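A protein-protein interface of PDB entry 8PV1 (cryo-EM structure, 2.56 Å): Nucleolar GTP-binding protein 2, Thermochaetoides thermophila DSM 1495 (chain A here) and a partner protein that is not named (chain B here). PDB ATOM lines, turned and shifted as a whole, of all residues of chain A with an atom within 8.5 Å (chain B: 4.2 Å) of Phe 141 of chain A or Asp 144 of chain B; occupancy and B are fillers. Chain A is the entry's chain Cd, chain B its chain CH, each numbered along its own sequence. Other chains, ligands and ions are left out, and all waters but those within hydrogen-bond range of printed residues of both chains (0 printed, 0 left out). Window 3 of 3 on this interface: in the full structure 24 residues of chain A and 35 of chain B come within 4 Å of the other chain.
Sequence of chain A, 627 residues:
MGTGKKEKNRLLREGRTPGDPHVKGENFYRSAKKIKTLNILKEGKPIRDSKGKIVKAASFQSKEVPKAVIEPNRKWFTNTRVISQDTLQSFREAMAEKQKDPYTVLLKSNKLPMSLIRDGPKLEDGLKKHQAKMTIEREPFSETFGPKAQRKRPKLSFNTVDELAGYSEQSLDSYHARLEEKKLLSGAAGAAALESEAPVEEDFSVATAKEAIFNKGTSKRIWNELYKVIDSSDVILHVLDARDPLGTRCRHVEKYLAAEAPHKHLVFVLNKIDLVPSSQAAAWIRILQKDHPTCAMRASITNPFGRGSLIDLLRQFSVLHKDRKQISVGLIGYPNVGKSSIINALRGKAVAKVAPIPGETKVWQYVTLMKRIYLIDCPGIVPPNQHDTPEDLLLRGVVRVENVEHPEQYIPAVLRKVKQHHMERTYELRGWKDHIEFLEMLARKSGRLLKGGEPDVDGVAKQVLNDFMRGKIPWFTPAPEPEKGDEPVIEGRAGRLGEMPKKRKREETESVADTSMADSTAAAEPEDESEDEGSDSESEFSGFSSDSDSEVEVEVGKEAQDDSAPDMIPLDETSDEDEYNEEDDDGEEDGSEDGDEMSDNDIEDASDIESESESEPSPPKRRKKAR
The side-chain hydroxyl of Thr 144 of chain A sits at hydrogen-bond distance from a ring nitrogen (NE2) of His 89 of chain B.
The backbone carbonyl oxygen (O) of Glu 139 of chain A sits at hydrogen-bond distance from a ring nitrogen (NE2) of His 89 of chain B, 2.7 Å away.
The backbone carbonyl oxygen (O) of Pro 140 of chain A lies within hydrogen-bond range of the side-chain hydroxyl (OG1) of Thr 144 of chain A, at 2.8 Å.
His 89 of chain B touches Ile 136 of chain A.
His 89 of chain B touches Pro 140 of chain A.
CE1 of Phe 141 of chain A touches O of His 89 of chain B (3.6 Å).
Ala 93 of chain B touches Phe 141 of chain A.
CD2 of Phe 141 of chain A touches CB of Asp 144 of chain B, 3.7 Å away.
Phe 141 of chain A touches Pro 145 of chain B.
Tyr 148 of chain B touches Phe 141 of chain A.
Tyr 148 of chain B touches Phe 145 of chain A.
Phe 141 of chain A touches just these residues of chain B: His 89, Ala 93, Asp 144, Pro 145 and Tyr 148.
Printed residues of chain B within 4 Å of Thr 144 of chain A: His 89.
Of the printed residues of chain A, His 89 of chain B touches Ile 136 (3.8 Å), Glu 139 (2.7 Å), Pro 140 (3.7 Å), Phe 141 (3.6 Å) and Thr 144 (3.3 Å).
Leu 142 of chain B touches none of the printed residues of chain A.
Asp 144 of chain B touches just one residue of chain A: Phe 141.
The nearest residue of chain A that does not touch Asp 144 of chain B is Ser 142 of chain A (5.7 Å).
The nearest printed residue of chain B that does not touch Phe 145 of chain A is Ile 147 of chain B (6.1 Å).
Of the 18 printed residues of chain A, 6 touch a printed residue of chain B.
Hydrophobic or aromatic side chains of chain A that line the printed part of chain B: Ile 136, Phe 141 and Phe 145.
Hydrophobic or aromatic side chains of chain B that line the printed part of chain A: His 89, Ala 93, Pro 145 and Tyr 148.
Among the printed residues, no Asp or Glu carboxylate lies within 4 Å of a Lys or Arg side-chain nitrogen of the other chain.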
ATOM      1  N   ALA A 132       3.401  -1.498   3.298  1.00  0.00           N
ATOM      2  CA  ALA A 132       2.256  -0.634   3.022  1.00  0.00           C
ATOM      3  C   ALA A 132       1.544  -1.041   1.736  1.00  0.00           C
ATOM      4  O   ALA A 132       0.321  -1.243   1.724  1.00  0.00           O
ATOM      5  CB  ALA A 132       2.706   0.824   2.951  1.00  0.00           C
ATOM      6  N   THR A 135      -0.218  -4.427   2.148  1.00  0.00           N
ATOM      7  CA  THR A 135      -1.523  -4.339   2.798  1.00  0.00           C
ATOM      8  C   THR A 135      -2.577  -3.755   1.863  1.00  0.00           C
ATOM      9  O   THR A 135      -3.728  -4.214   1.852  1.00  0.00           O
ATOM     10  CB  THR A 135      -1.428  -3.502   4.074  1.00  0.00           C
ATOM     11  OG1 THR A 135      -0.808  -2.246   3.779  1.00  0.00           O
ATOM     12  CG2 THR A 135      -0.620  -4.230   5.134  1.00  0.00           C
ATOM     13  N   ILE A 136      -2.206  -2.744   1.072  1.00  0.00           N
ATOM     14  CA  ILE A 136      -3.173  -2.151   0.148  1.00  0.00           C
ATOM     15  C   ILE A 136      -3.554  -3.137  -0.957  1.00  0.00           C
ATOM     16  O   ILE A 136      -4.720  -3.197  -1.369  1.00  0.00           O
ATOM     17  CB  ILE A 136      -2.627  -0.824  -0.415  1.00  0.00           C
ATOM     18  CG1 ILE A 136      -2.385   0.171   0.719  1.00  0.00           C
ATOM     19  CG2 ILE A 136      -3.595  -0.205  -1.412  1.00  0.00           C
ATOM     20  CD1 ILE A 136      -3.580   0.376   1.625  1.00  0.00           C
ATOM     21  N   GLU A 137      -2.596  -3.935  -1.439  1.00  0.00           N
ATOM     22  CA  GLU A 137      -2.907  -4.971  -2.419  1.00  0.00           C
ATOM     23  C   GLU A 137      -3.772  -6.069  -1.817  1.00  0.00           C
ATOM     24  O   GLU A 137      -4.667  -6.596  -2.489  1.00  0.00           O
ATOM     25  CB  GLU A 137      -1.618  -5.568  -2.981  1.00  0.00           C
ATOM     26  CG  GLU A 137      -0.929  -4.715  -4.025  1.00  0.00           C
ATOM     27  CD  GLU A 137       0.455  -5.228  -4.372  1.00  0.00           C
ATOM     28  OE1 GLU A 137       0.983  -6.074  -3.619  1.00  0.00           O
ATOM     29  OE2 GLU A 137       1.016  -4.786  -5.396  1.00  0.00           O
ATOM     30  N   ARG A 138      -3.507  -6.444  -0.562  1.00  0.00           N
ATOM     31  CA  ARG A 138      -4.298  -7.485   0.086  1.00  0.00           C
ATOM     32  C   ARG A 138      -5.739  -7.046   0.299  1.00  0.00           C
ATOM     33  O   ARG A 138      -6.671  -7.818   0.053  1.00  0.00           O
ATOM     34  CB  ARG A 138      -3.661  -7.875   1.417  1.00  0.00           C
ATOM     35  CG  ARG A 138      -4.389  -8.989   2.141  1.00  0.00           C
ATOM     36  CD  ARG A 138      -4.011  -9.066   3.612  1.00  0.00           C
ATOM     37  NE  ARG A 138      -2.585  -8.865   3.839  1.00  0.00           N
ATOM     38  CZ  ARG A 138      -2.064  -7.830   4.482  1.00  0.00           C
ATOM     39  NH1 ARG A 138      -2.828  -6.875   4.986  1.00  0.00           N
ATOM     40  NH2 ARG A 138      -0.745  -7.749   4.622  1.00  0.00           N
ATOM     41  N   GLU A 139      -5.946  -5.815   0.758  1.00  0.00           N
ATOM     42  CA  GLU A 139      -7.291  -5.291   0.985  1.00  0.00           C
ATOM     43  C   GLU A 139      -7.333  -3.786   0.727  1.00  0.00           C
ATOM     44  O   GLU A 139      -6.609  -3.009   1.375  1.00  0.00           O
ATOM     45  CB  GLU A 139      -7.788  -5.700   2.374  1.00  0.00           C
ATOM     46  CG  GLU A 139      -7.048  -5.152   3.579  1.00  0.00           C
ATOM     47  CD  GLU A 139      -7.587  -5.680   4.895  1.00  0.00           C
ATOM     48  OE1 GLU A 139      -8.531  -6.497   4.868  1.00  0.00           O
ATOM     49  OE2 GLU A 139      -7.060  -5.286   5.957  1.00  0.00           O
ATOM     50  N   PRO A 140      -8.104  -3.347  -0.268  1.00  0.00           N
ATOM     51  CA  PRO A 140      -8.062  -1.936  -0.670  1.00  0.00           C
ATOM     52  C   PRO A 140      -8.786  -1.027   0.310  1.00  0.00           C
ATOM     53  O   PRO A 140      -9.418  -1.478   1.267  1.00  0.00           O
ATOM     54  CB  PRO A 140      -8.755  -1.930  -2.039  1.00  0.00           C
ATOM     55  CG  PRO A 140      -9.474  -3.220  -2.135  1.00  0.00           C
ATOM     56  CD  PRO A 140      -8.766  -4.197  -1.271  1.00  0.00           C
ATOM     57  N   PHE A 141      -8.676   0.279   0.049  1.00  0.00           N
ATOM     58  CA  PHE A 141      -9.306   1.285   0.899  1.00  0.00           C
ATOM     59  C   PHE A 141     -10.825   1.183   0.858  1.00  0.00           C
ATOM     60  O   PHE A 141     -11.493   1.344   1.885  1.00  0.00           O
ATOM     61  CB  PHE A 141      -8.863   2.683   0.469  1.00  0.00           C
ATOM     62  CG  PHE A 141      -7.495   3.065   0.947  1.00  0.00           C
ATOM     63  CD1 PHE A 141      -7.264   3.341   2.283  1.00  0.00           C
ATOM     64  CD2 PHE A 141      -6.440   3.154   0.058  1.00  0.00           C
ATOM     65  CE1 PHE A 141      -6.007   3.699   2.723  1.00  0.00           C
ATOM     66  CE2 PHE A 141      -5.179   3.506   0.492  1.00  0.00           C
ATOM     67  CZ  PHE A 141      -4.963   3.780   1.826  1.00  0.00           C
ATOM     68  N   SER A 142     -11.389   0.934  -0.326  1.00  0.00           N
ATOM     69  CA  SER A 142     -12.838   0.911  -0.486  1.00  0.00           C
ATOM     70  C   SER A 142     -13.489  -0.281   0.203  1.00  0.00           C
ATOM     71  O   SER A 142     -14.643  -0.177   0.631  1.00  0.00           O
ATOM     72  CB  SER A 142     -13.199   0.911  -1.969  1.00  0.00           C
ATOM     73  OG  SER A 142     -12.623  -0.200  -2.628  1.00  0.00           O
ATOM     74  N   GLU A 143     -12.786  -1.405   0.315  1.00  0.00           N
ATOM     75  CA  GLU A 143     -13.317  -2.573   1.001  1.00  0.00           C
ATOM     76  C   GLU A 143     -13.112  -2.523   2.507  1.00  0.00           C
ATOM     77  O   GLU A 143     -13.652  -3.374   3.219  1.00  0.00           O
ATOM     78  CB  GLU A 143     -12.674  -3.848   0.449  1.00  0.00           C
ATOM     79  CG  GLU A 143     -12.946  -4.093  -1.021  1.00  0.00           C
ATOM     80  CD  GLU A 143     -12.270  -5.347  -1.532  1.00  0.00           C
ATOM     81  OE1 GLU A 143     -11.535  -5.986  -0.750  1.00  0.00           O
ATOM     82  OE2 GLU A 143     -12.469  -5.693  -2.715  1.00  0.00           O
ATOM     83  N   THR A 144     -12.349  -1.553   3.006  1.00  0.00           N
ATOM     84  CA  THR A 144     -12.069  -1.451   4.431  1.00  0.00           C
ATOM     85  C   THR A 144     -13.061  -0.540   5.145  1.00  0.00           C
ATOM     86  O   THR A 144     -13.683  -0.949   6.130  1.00  0.00           O
ATOM     87  CB  THR A 144     -10.640  -0.949   4.647  1.00  0.00           C
ATOM     88  OG1 THR A 144      -9.717  -1.860   4.039  1.00  0.00           O
ATOM     89  CG2 THR A 144     -10.340  -0.846   6.118  1.00  0.00           C
ATOM     90  N   PHE A 145     -13.218   0.690   4.665  1.00  0.00           N
ATOM     91  CA  PHE A 145     -14.148   1.635   5.259  1.00  0.00           C
ATOM     92  C   PHE A 145     -14.845   2.415   4.155  1.00  0.00           C
ATOM     93  O   PHE A 145     -14.226   2.795   3.157  1.00  0.00           O
ATOM     94  CB  PHE A 145     -13.438   2.594   6.222  1.00  0.00           C
ATOM     95  CG  PHE A 145     -14.369   3.338   7.132  1.00  0.00           C
ATOM     96  CD1 PHE A 145     -14.880   2.731   8.266  1.00  0.00           C
ATOM     97  CD2 PHE A 145     -14.738   4.642   6.851  1.00  0.00           C
ATOM     98  CE1 PHE A 145     -15.739   3.411   9.102  1.00  0.00           C
ATOM     99  CE2 PHE A 145     -15.595   5.327   7.685  1.00  0.00           C
ATOM    100  CZ  PHE A 145     -16.097   4.711   8.811  1.00  0.00           C
ATOM    101  N   GLY A 146     -16.139   2.652   4.341  1.00  0.00           N
ATOM    102  CA  GLY A 146     -16.920   3.391   3.379  1.00  0.00           C
ATOM    103  C   GLY A 146     -18.270   2.758   3.118  1.00  0.00           C
ATOM    104  O   GLY A 146     -18.675   1.804   3.788  1.00  0.00           O
ATOM    105  N   PRO A 147     -19.002   3.292   2.136  1.00  0.00           N
ATOM    106  CA  PRO A 147     -20.338   2.751   1.834  1.00  0.00           C
ATOM    107  C   PRO A 147     -20.323   1.358   1.226  1.00  0.00           C
ATOM    108  O   PRO A 147     -21.356   0.679   1.257  1.00  0.00           O
ATOM    109  CB  PRO A 147     -20.919   3.780   0.854  1.00  0.00           C
ATOM    110  CG  PRO A 147     -19.731   4.451   0.261  1.00  0.00           C
ATOM    111  CD  PRO A 147     -18.696   4.490   1.338  1.00  0.00           C
ATOM    112  N   LYS A 148     -19.196   0.911   0.668  1.00  0.00           N
ATOM    113  CA  LYS A 148     -19.097  -0.411   0.061  1.00  0.00           C
ATOM    114  C   LYS A 148     -18.093  -1.300   0.786  1.00  0.00           C
ATOM    115  O   LYS A 148     -17.560  -2.241   0.189  1.00  0.00           O
ATOM    116  CB  LYS A 148     -18.725  -0.299  -1.419  1.00  0.00           C
ATOM    117  CG  LYS A 148     -19.618   0.624  -2.230  1.00  0.00           C
ATOM    118  CD  LYS A 148     -21.086   0.273  -2.080  1.00  0.00           C
ATOM    119  CE  LYS A 148     -21.968   1.343  -2.700  1.00  0.00           C
ATOM    120  NZ  LYS A 148     -23.411   1.107  -2.424  1.00  0.00           N
ATOM    121  N   ALA A 149     -17.817  -1.013   2.056  1.00  0.00           N
ATOM    122  CA  ALA A 149     -16.829  -1.778   2.802  1.00  0.00           C
ATOM    123  C   ALA A 149     -17.343  -3.176   3.118  1.00  0.00           C
ATOM    124  O   ALA A 149     -18.508  -3.372   3.475  1.00  0.00           O
ATOM    125  CB  ALA A 149     -16.469  -1.055   4.098  1.00  0.00           C
ATOM    126  N   GLN A 150     -16.453  -4.157   2.985  1.00  0.00           N
ATOM    127  CA  GLN A 150     -16.764  -5.543   3.291  1.00  0.00           C
ATOM    128  C   GLN A 150     -15.977  -6.076   4.478  1.00  0.00           C
ATOM    129  O   GLN A 150     -16.041  -7.279   4.753  1.00  0.00           O
ATOM    130  CB  GLN A 150     -16.510  -6.430   2.066  1.00  0.00           C
ATOM    131  CG  GLN A 150     -17.337  -6.057   0.851  1.00  0.00           C
ATOM    132  CD  GLN A 150     -18.822  -6.243   1.077  1.00  0.00           C
ATOM    133  OE1 GLN A 150     -19.276  -7.329   1.431  1.00  0.00           O
ATOM    134  NE2 GLN A 150     -19.591  -5.182   0.868  1.00  0.00           N
ATOM    135  N   ARG A 151     -15.238  -5.223   5.180  1.00  0.00           N
ATOM    136  CA  ARG A 151     -14.434  -5.666   6.310  1.00  0.00           C
ATOM    137  C   ARG A 151     -15.323  -5.972   7.508  1.00  0.00           C
ATOM    138  O   ARG A 151     -16.150  -5.147   7.909  1.00  0.00           O
ATOM    139  CB  ARG A 151     -13.408  -4.591   6.662  1.00  0.00           C
ATOM    140  CG  ARG A 151     -12.732  -4.758   8.007  1.00  0.00           C
ATOM    141  CD  ARG A 151     -11.717  -3.653   8.216  1.00  0.00           C
ATOM    142  NE  ARG A 151     -11.052  -3.726   9.509  1.00  0.00           N
ATOM    143  CZ  ARG A 151     -11.423  -3.041  10.582  1.00  0.00           C
ATOM    144  NH1 ARG A 151     -12.472  -2.236  10.560  1.00  0.00           N
ATOM    145  NH2 ARG A 151     -10.722  -3.166  11.705  1.00  0.00           N
ATOM    146  N   HIS B  89      -4.435   0.824   7.676  1.00  0.00           N
ATOM    147  CA  HIS B  89      -4.881   1.629   6.539  1.00  0.00           C
ATOM    148  C   HIS B  89      -4.840   3.116   6.855  1.00  0.00           C
ATOM    149  O   HIS B  89      -4.505   3.933   5.989  1.00  0.00           O
ATOM    150  CB  HIS B  89      -6.294   1.221   6.127  1.00  0.00           C
ATOM    151  CG  HIS B  89      -6.334   0.066   5.184  1.00  0.00           C
ATOM    152  ND1 HIS B  89      -6.039  -1.221   5.573  1.00  0.00           N
ATOM    153  CD2 HIS B  89      -6.626   0.004   3.864  1.00  0.00           C
ATOM    154  CE1 HIS B  89      -6.148  -2.027   4.534  1.00  0.00           C
ATOM    155  NE2 HIS B  89      -6.507  -1.310   3.485  1.00  0.00           N
ATOM    156  N   ALA B  93      -2.553   5.681   4.696  1.00  0.00           N
ATOM    157  CA  ALA B  93      -3.154   6.807   3.984  1.00  0.00           C
ATOM    158  C   ALA B  93      -2.492   8.128   4.364  1.00  0.00           C
ATOM    159  O   ALA B  93      -2.150   8.944   3.492  1.00  0.00           O
ATOM    160  CB  ALA B  93      -4.655   6.853   4.264  1.00  0.00           C
ATOM    161  N   LEU B 142      -3.468   9.746  -5.609  1.00  0.00           N
ATOM    162  CA  LEU B 142      -3.998   9.667  -4.254  1.00  0.00           C
ATOM    163  C   LEU B 142      -5.511   9.500  -4.212  1.00  0.00           C
ATOM    164  O   LEU B 142      -6.140   9.995  -3.275  1.00  0.00           O
ATOM    165  CB  LEU B 142      -3.619  10.916  -3.460  1.00  0.00           C
ATOM    166  CG  LEU B 142      -2.170  11.172  -3.067  1.00  0.00           C
ATOM    167  CD1 LEU B 142      -2.064  12.560  -2.478  1.00  0.00           C
ATOM    168  CD2 LEU B 142      -1.694  10.133  -2.072  1.00  0.00           C
ATOM    169  N   LYS B 143      -6.109   8.827  -5.195  1.00  0.00           N
ATOM    170  CA  LYS B 143      -7.565   8.812  -5.316  1.00  0.00           C
ATOM    171  C   LYS B 143      -8.232   8.049  -4.172  1.00  0.00           C
ATOM    172  O   LYS B 143      -9.180   8.541  -3.551  1.00  0.00           O
ATOM    173  CB  LYS B 143      -7.963   8.215  -6.665  1.00  0.00           C
ATOM    174  CG  LYS B 143      -9.454   8.203  -6.916  1.00  0.00           C
ATOM    175  CD  LYS B 143      -9.776   7.704  -8.309  1.00  0.00           C
ATOM    176  CE  LYS B 143     -11.276   7.554  -8.500  1.00  0.00           C
ATOM    177  NZ  LYS B 143     -11.981   8.865  -8.450  1.00  0.00           N
ATOM    178  N   ASP B 144      -7.743   6.844  -3.875  1.00  0.00           N
ATOM    179  CA  ASP B 144      -8.376   6.029  -2.836  1.00  0.00           C
ATOM    180  C   ASP B 144      -8.092   6.514  -1.413  1.00  0.00           C
ATOM    181  O   ASP B 144      -9.028   6.501  -0.589  1.00  0.00           O
ATOM    182  CB  ASP B 144      -7.988   4.559  -3.030  1.00  0.00           C
ATOM    183  CG  ASP B 144      -8.242   4.074  -4.441  1.00  0.00           C
ATOM    184  OD1 ASP B 144      -9.121   4.644  -5.118  1.00  0.00           O
ATOM    185  OD2 ASP B 144      -7.557   3.126  -4.877  1.00  0.00           O
ATOM    186  N   PRO B 145      -6.853   6.919  -1.033  1.00  0.00           N
ATOM    187  CA  PRO B 145      -6.668   7.468   0.324  1.00  0.00           C
ATOM    188  C   PRO B 145      -7.505   8.694   0.639  1.00  0.00           C
ATOM    189  O   PRO B 145      -7.936   8.840   1.784  1.00  0.00           O
ATOM    190  CB  PRO B 145      -5.171   7.800   0.363  1.00  0.00           C
ATOM    191  CG  PRO B 145      -4.566   6.862  -0.547  1.00  0.00           C
ATOM    192  CD  PRO B 145      -5.534   6.694  -1.666  1.00  0.00           C
ATOM    193  N   LEU B 146      -7.762   9.570  -0.336  1.00  0.00           N
ATOM    194  CA  LEU B 146      -8.534  10.778  -0.056  1.00  0.00           C
ATOM    195  C   LEU B 146      -9.991  10.448   0.252  1.00  0.00           C
ATOM    196  O   LEU B 146     -10.589  11.019   1.173  1.00  0.00           O
ATOM    197  CB  LEU B 146      -8.425  11.748  -1.232  1.00  0.00           C
ATOM    198  CG  LEU B 146      -7.064  12.437  -1.363  1.00  0.00           C
ATOM    199  CD1 LEU B 146      -6.980  13.263  -2.634  1.00  0.00           C
ATOM    200  CD2 LEU B 146      -6.755  13.286  -0.145  1.00  0.00           C
ATOM    201  N   ILE B 147     -10.573   9.509  -0.499  1.00  0.00           N
ATOM    202  CA  ILE B 147     -11.948   9.077  -0.245  1.00  0.00           C
ATOM    203  C   ILE B 147     -12.045   8.385   1.110  1.00  0.00           C
ATOM    204  O   ILE B 147     -12.967   8.642   1.904  1.00  0.00           O
ATOM    205  CB  ILE B 147     -12.432   8.159  -1.381  1.00  0.00           C
ATOM    206  CG1 ILE B 147     -12.406   8.903  -2.715  1.00  0.00           C
ATOM    207  CG2 ILE B 147     -13.826   7.634  -1.095  1.00  0.00           C
ATOM    208  CD1 ILE B 147     -12.553   7.998  -3.909  1.00  0.00           C
ATOM    209  N   TYR B 148     -11.077   7.503   1.395  1.00  0.00           N
ATOM    210  CA  TYR B 148     -11.046   6.812   2.680  1.00  0.00           C
ATOM    211  C   TYR B 148     -10.914   7.794   3.838  1.00  0.00           C
ATOM    212  O   TYR B 148     -11.608   7.664   4.855  1.00  0.00           O
ATOM    213  CB  TYR B 148      -9.897   5.801   2.686  1.00  0.00           C
ATOM    214  CG  TYR B 148      -9.523   5.252   4.043  1.00  0.00           C
ATOM    215  CD1 TYR B 148     -10.225   4.195   4.604  1.00  0.00           C
ATOM    216  CD2 TYR B 148      -8.441   5.767   4.747  1.00  0.00           C
ATOM    217  CE1 TYR B 148      -9.877   3.684   5.840  1.00  0.00           C
ATOM    218  CE2 TYR B 148      -8.089   5.264   5.980  1.00  0.00           C
ATOM    219  CZ  TYR B 148      -8.807   4.225   6.521  1.00  0.00           C
ATOM    220  OH  TYR B 148      -8.450   3.724   7.749  1.00  0.00           O
